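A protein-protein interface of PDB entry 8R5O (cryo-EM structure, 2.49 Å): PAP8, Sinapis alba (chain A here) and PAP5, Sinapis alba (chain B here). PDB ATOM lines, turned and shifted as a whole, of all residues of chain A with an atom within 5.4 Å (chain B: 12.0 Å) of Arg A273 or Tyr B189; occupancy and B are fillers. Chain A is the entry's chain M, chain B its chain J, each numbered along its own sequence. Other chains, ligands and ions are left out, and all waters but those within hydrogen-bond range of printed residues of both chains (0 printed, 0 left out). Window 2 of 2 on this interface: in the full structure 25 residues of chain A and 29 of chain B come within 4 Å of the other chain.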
ATOM      1  N   GLU A 248       3.592  21.538  14.133  1.00  0.00           N
ATOM      2  CA  GLU A 248       2.699  21.167  15.224  1.00  0.00           C
ATOM      3  C   GLU A 248       1.390  21.942  15.194  1.00  0.00           C
ATOM      4  O   GLU A 248       0.423  21.521  15.837  1.00  0.00           O
ATOM      5  CB  GLU A 248       3.395  21.378  16.569  1.00  0.00           C
ATOM      6  CG  GLU A 248       4.646  20.540  16.758  1.00  0.00           C
ATOM      7  CD  GLU A 248       5.377  20.868  18.043  1.00  0.00           C
ATOM      8  OE1 GLU A 248       4.865  21.695  18.827  1.00  0.00           O
ATOM      9  OE2 GLU A 248       6.467  20.302  18.267  1.00  0.00           O
ATOM     10  N   LEU A 266       1.054  13.679  14.740  1.00  0.00           N
ATOM     11  CA  LEU A 266       1.830  12.723  15.518  1.00  0.00           C
ATOM     12  C   LEU A 266       3.310  12.995  15.286  1.00  0.00           C
ATOM     13  O   LEU A 266       3.768  13.016  14.140  1.00  0.00           O
ATOM     14  CB  LEU A 266       1.478  11.288  15.126  1.00  0.00           C
ATOM     15  CG  LEU A 266       2.303  10.177  15.778  1.00  0.00           C
ATOM     16  CD1 LEU A 266       2.054  10.128  17.277  1.00  0.00           C
ATOM     17  CD2 LEU A 266       1.995   8.836  15.134  1.00  0.00           C
ATOM     18  N   VAL A 267       4.051  13.202  16.368  1.00  0.00           N
ATOM     19  CA  VAL A 267       5.472  13.517  16.296  1.00  0.00           C
ATOM     20  C   VAL A 267       6.258  12.268  16.665  1.00  0.00           C
ATOM     21  O   VAL A 267       6.153  11.767  17.790  1.00  0.00           O
ATOM     22  CB  VAL A 267       5.836  14.689  17.221  1.00  0.00           C
ATOM     23  CG1 VAL A 267       7.293  15.074  17.037  1.00  0.00           C
ATOM     24  CG2 VAL A 267       4.924  15.876  16.961  1.00  0.00           C
ATOM     25  N   GLY A 271      13.240  14.144  20.611  1.00  0.00           N
ATOM     26  CA  GLY A 271      13.602  15.481  21.030  1.00  0.00           C
ATOM     27  C   GLY A 271      12.478  16.208  21.737  1.00  0.00           C
ATOM     28  O   GLY A 271      12.717  17.178  22.462  1.00  0.00           O
ATOM     29  N   GLY A 272      11.246  15.742  21.543  1.00  0.00           N
ATOM     30  CA  GLY A 272      10.117  16.379  22.190  1.00  0.00           C
ATOM     31  C   GLY A 272       9.854  17.773  21.644  1.00  0.00           C
ATOM     32  O   GLY A 272      10.068  18.064  20.464  1.00  0.00           O
ATOM     33  N   ARG A 273       9.375  18.650  22.529  1.00  0.00           N
ATOM     34  CA  ARG A 273       9.020  20.003  22.111  1.00  0.00           C
ATOM     35  C   ARG A 273      10.254  20.813  21.733  1.00  0.00           C
ATOM     36  O   ARG A 273      10.206  21.627  20.804  1.00  0.00           O
ATOM     37  CB  ARG A 273       8.232  20.705  23.217  1.00  0.00           C
ATOM     38  CG  ARG A 273       6.971  19.970  23.633  1.00  0.00           C
ATOM     39  CD  ARG A 273       6.030  20.875  24.413  1.00  0.00           C
ATOM     40  NE  ARG A 273       4.815  20.175  24.812  1.00  0.00           N
ATOM     41  CZ  ARG A 273       3.733  20.767  25.298  1.00  0.00           C
ATOM     42  NH1 ARG A 273       3.673  22.080  25.452  1.00  0.00           N
ATOM     43  NH2 ARG A 273       2.682  20.024  25.635  1.00  0.00           N
ATOM     44  N   LYS A 274      11.364  20.609  22.438  1.00  0.00           N
ATOM     45  CA  LYS A 274      12.617  21.306  22.151  1.00  0.00           C
ATOM     46  C   LYS A 274      13.464  20.412  21.253  1.00  0.00           C
ATOM     47  O   LYS A 274      14.119  19.479  21.723  1.00  0.00           O
ATOM     48  CB  LYS A 274      13.354  21.666  23.436  1.00  0.00           C
ATOM     49  CG  LYS A 274      12.859  22.940  24.097  1.00  0.00           C
ATOM     50  CD  LYS A 274      13.777  23.364  25.231  1.00  0.00           C
ATOM     51  CE  LYS A 274      13.350  24.697  25.817  1.00  0.00           C
ATOM     52  NZ  LYS A 274      14.249  25.127  26.921  1.00  0.00           N
ATOM     53  N   ARG A 275      13.454  20.707  19.957  1.00  0.00           N
ATOM     54  CA  ARG A 275      14.206  19.934  18.983  1.00  0.00           C
ATOM     55  C   ARG A 275      14.604  20.855  17.842  1.00  0.00           C
ATOM     56  O   ARG A 275      14.092  21.968  17.705  1.00  0.00           O
ATOM     57  CB  ARG A 275      13.392  18.747  18.459  1.00  0.00           C
ATOM     58  CG  ARG A 275      12.213  19.153  17.588  1.00  0.00           C
ATOM     59  CD  ARG A 275      11.364  17.959  17.195  1.00  0.00           C
ATOM     60  NE  ARG A 275      10.253  18.349  16.337  1.00  0.00           N
ATOM     61  CZ  ARG A 275       9.090  18.807  16.777  1.00  0.00           C
ATOM     62  NH1 ARG A 275       8.847  18.946  18.070  1.00  0.00           N
ATOM     63  NH2 ARG A 275       8.148  19.138  15.900  1.00  0.00           N
ATOM     64  N   ARG A 277      14.031  22.018  14.604  1.00  0.00           N
ATOM     65  CA  ARG A 277      12.940  21.998  13.640  1.00  0.00           C
ATOM     66  C   ARG A 277      13.431  21.936  12.201  1.00  0.00           C
ATOM     67  O   ARG A 277      12.620  21.715  11.298  1.00  0.00           O
ATOM     68  CB  ARG A 277      12.053  23.229  13.826  1.00  0.00           C
ATOM     69  CG  ARG A 277      11.503  23.395  15.230  1.00  0.00           C
ATOM     70  CD  ARG A 277      10.164  22.701  15.396  1.00  0.00           C
ATOM     71  NE  ARG A 277       9.556  23.008  16.684  1.00  0.00           N
ATOM     72  CZ  ARG A 277       8.282  22.795  16.980  1.00  0.00           C
ATOM     73  NH1 ARG A 277       7.445  22.276  16.097  1.00  0.00           N
ATOM     74  NH2 ARG A 277       7.835  23.117  18.190  1.00  0.00           N
ATOM     75  N   ASN B 184      -3.392  22.057  22.530  1.00  0.00           N
ATOM     76  CA  ASN B 184      -4.343  21.278  23.313  1.00  0.00           C
ATOM     77  C   ASN B 184      -4.056  19.786  23.183  1.00  0.00           C
ATOM     78  O   ASN B 184      -2.961  19.326  23.503  1.00  0.00           O
ATOM     79  CB  ASN B 184      -5.776  21.581  22.874  1.00  0.00           C
ATOM     80  CG  ASN B 184      -6.092  23.064  22.900  1.00  0.00           C
ATOM     81  OD1 ASN B 184      -5.411  23.845  23.566  1.00  0.00           O
ATOM     82  ND2 ASN B 184      -7.132  23.460  22.176  1.00  0.00           N
ATOM     83  N   GLY B 185      -5.048  19.034  22.717  1.00  0.00           N
ATOM     84  CA  GLY B 185      -4.877  17.611  22.505  1.00  0.00           C
ATOM     85  C   GLY B 185      -4.662  17.257  21.049  1.00  0.00           C
ATOM     86  O   GLY B 185      -5.182  16.248  20.564  1.00  0.00           O
ATOM     87  N   PHE B 186      -3.891  18.083  20.338  1.00  0.00           N
ATOM     88  CA  PHE B 186      -3.671  17.898  18.912  1.00  0.00           C
ATOM     89  C   PHE B 186      -2.264  17.449  18.554  1.00  0.00           C
ATOM     90  O   PHE B 186      -2.045  17.015  17.421  1.00  0.00           O
ATOM     91  CB  PHE B 186      -3.991  19.195  18.153  1.00  0.00           C
ATOM     92  CG  PHE B 186      -5.453  19.523  18.116  1.00  0.00           C
ATOM     93  CD1 PHE B 186      -6.267  18.983  17.136  1.00  0.00           C
ATOM     94  CD2 PHE B 186      -6.017  20.357  19.065  1.00  0.00           C
ATOM     95  CE1 PHE B 186      -7.613  19.272  17.099  1.00  0.00           C
ATOM     96  CE2 PHE B 186      -7.365  20.650  19.032  1.00  0.00           C
ATOM     97  CZ  PHE B 186      -8.163  20.107  18.049  1.00  0.00           C
ATOM     98  N   VAL B 187      -1.315  17.534  19.481  1.00  0.00           N
ATOM     99  CA  VAL B 187       0.057  17.098  19.255  1.00  0.00           C
ATOM    100  C   VAL B 187       0.331  15.908  20.162  1.00  0.00           C
ATOM    101  O   VAL B 187       0.152  15.994  21.384  1.00  0.00           O
ATOM    102  CB  VAL B 187       1.060  18.235  19.513  1.00  0.00           C
ATOM    103  CG1 VAL B 187       2.460  17.810  19.112  1.00  0.00           C
ATOM    104  CG2 VAL B 187       0.640  19.489  18.763  1.00  0.00           C
ATOM    105  N   VAL B 188       0.759  14.798  19.567  1.00  0.00           N
ATOM    106  CA  VAL B 188       1.059  13.569  20.290  1.00  0.00           C
ATOM    107  C   VAL B 188       2.497  13.178  19.986  1.00  0.00           C
ATOM    108  O   VAL B 188       2.902  13.141  18.819  1.00  0.00           O
ATOM    109  CB  VAL B 188       0.091  12.433  19.910  1.00  0.00           C
ATOM    110  CG1 VAL B 188       0.520  11.132  20.564  1.00  0.00           C
ATOM    111  CG2 VAL B 188      -1.329  12.791  20.311  1.00  0.00           C
ATOM    112  N   TYR B 189       3.264  12.888  21.034  1.00  0.00           N
ATOM    113  CA  TYR B 189       4.661  12.495  20.909  1.00  0.00           C
ATOM    114  C   TYR B 189       4.802  11.011  21.210  1.00  0.00           C
ATOM    115  O   TYR B 189       4.285  10.525  22.220  1.00  0.00           O
ATOM    116  CB  TYR B 189       5.546  13.306  21.855  1.00  0.00           C
ATOM    117  CG  TYR B 189       5.505  14.794  21.609  1.00  0.00           C
ATOM    118  CD1 TYR B 189       4.576  15.598  22.254  1.00  0.00           C
ATOM    119  CD2 TYR B 189       6.396  15.396  20.733  1.00  0.00           C
ATOM    120  CE1 TYR B 189       4.535  16.957  22.032  1.00  0.00           C
ATOM    121  CE2 TYR B 189       6.363  16.755  20.506  1.00  0.00           C
ATOM    122  CZ  TYR B 189       5.431  17.530  21.156  1.00  0.00           C
ATOM    123  OH  TYR B 189       5.394  18.887  20.932  1.00  0.00           O
ATOM    124  N   ASN B 190       5.503  10.297  20.334  1.00  0.00           N
ATOM    125  CA  ASN B 190       5.774   8.881  20.545  1.00  0.00           C
ATOM    126  C   ASN B 190       7.162   8.512  20.034  1.00  0.00           C
ATOM    127  O   ASN B 190       7.456   7.340  19.794  1.00  0.00           O
ATOM    128  CB  ASN B 190       4.712   8.019  19.856  1.00  0.00           C
ATOM    129  CG  ASN B 190       4.796   8.086  18.346  1.00  0.00           C
ATOM    130  OD1 ASN B 190       5.196   9.101  17.776  1.00  0.00           O
ATOM    131  ND2 ASN B 190       4.414   6.999  17.685  1.00  0.00           N
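Among the printed residues, pairs that only touch across the chains: Glu A248 with Val B187 (3.6 Å), Leu A266 with Val B188 (3.5 Å), Leu A266 with Asn B190 (3.3 Å), Val A267 with Val B187 (3.8 Å), Val A267 with Tyr B189 (3.5 Å), Gly A272 with Tyr B189 (3.8 Å) and Arg A273 with Tyr B189 (3.3 Å).
OE2 of Glu A248 lies within salt-bridge range of NH1 of Arg A275 (2.7 Å). NH1 of Arg A277 is in salt-bridge range of OE2 of Glu A248 (3.1 Å). The backbone carbonyl oxygen (O) of Gly A272 lies within hydrogen-bond range of the guanidinium group (NH1) of Arg A275.
Hydrophobic or aromatic side chains of chain A within 4 Å of the printed part of chain B: Leu A266 and Val A267. Among the printed residues, 10 pairs touch across the chains. Among the printed residues, no Asp or Glu carboxylate lies within 4 Å of a Lys or Arg side-chain nitrogen of the other chain.
Arg A273 touches just one residue of chain B: Tyr B189 (3.3 Å). Of chain A, only Glu A248, Val A267, Gly A272 and Arg A273 come within 4 Å of Tyr B189. Of chain B, only Val B187 (3.6 Å) and Tyr B189 (3.2 Å) come within 4 Å of Glu A248. Val A267 touches four residues of chain B. No residue of chain B comes within 4 Å of Gly A271. Of chain B, only Tyr B189 (3.8 Å) comes within 4 Å of Gly A272. Arg A275 touches none of the printed residues of chain B. Printed residues of chain A within 4 Å of Val B187: Glu A248 and Val A267. Printed residues of chain A within 4 Å of Asn B190: Leu A266 (3.3 Å) and Val A267 (2.8 Å). Printed residues of chain A within 4 Å of Val B188: Leu A266 (3.5 Å) and Val A267 (2.7 Å). Arg A277 touches none of the printed residues of chain B. Phe B186 touches none of the printed residues of chain A. The nearest residue of chain B that does not touch Arg A273 is Asn B184 (6.1 Å). The nearest residue of chain A that does not touch Tyr B189 is Arg A275 (4.1 Å). The nearest printed residue of chain A that does not touch Asn B190 is Gly A272 (7.9 Å).
The side-chain carboxylate (OE2) of Glu A248 is in hydrogen-bond range of the side-chain hydroxyl (OH) of Tyr B189, at 3.2 Å. The backbone NH (N) of Val A267 lies within hydrogen-bond range of the backbone carbonyl oxygen (O) of Val B188, at 2.7 Å. O of Val A267 lies close to OD1 of Asn B190 (2.8 Å).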
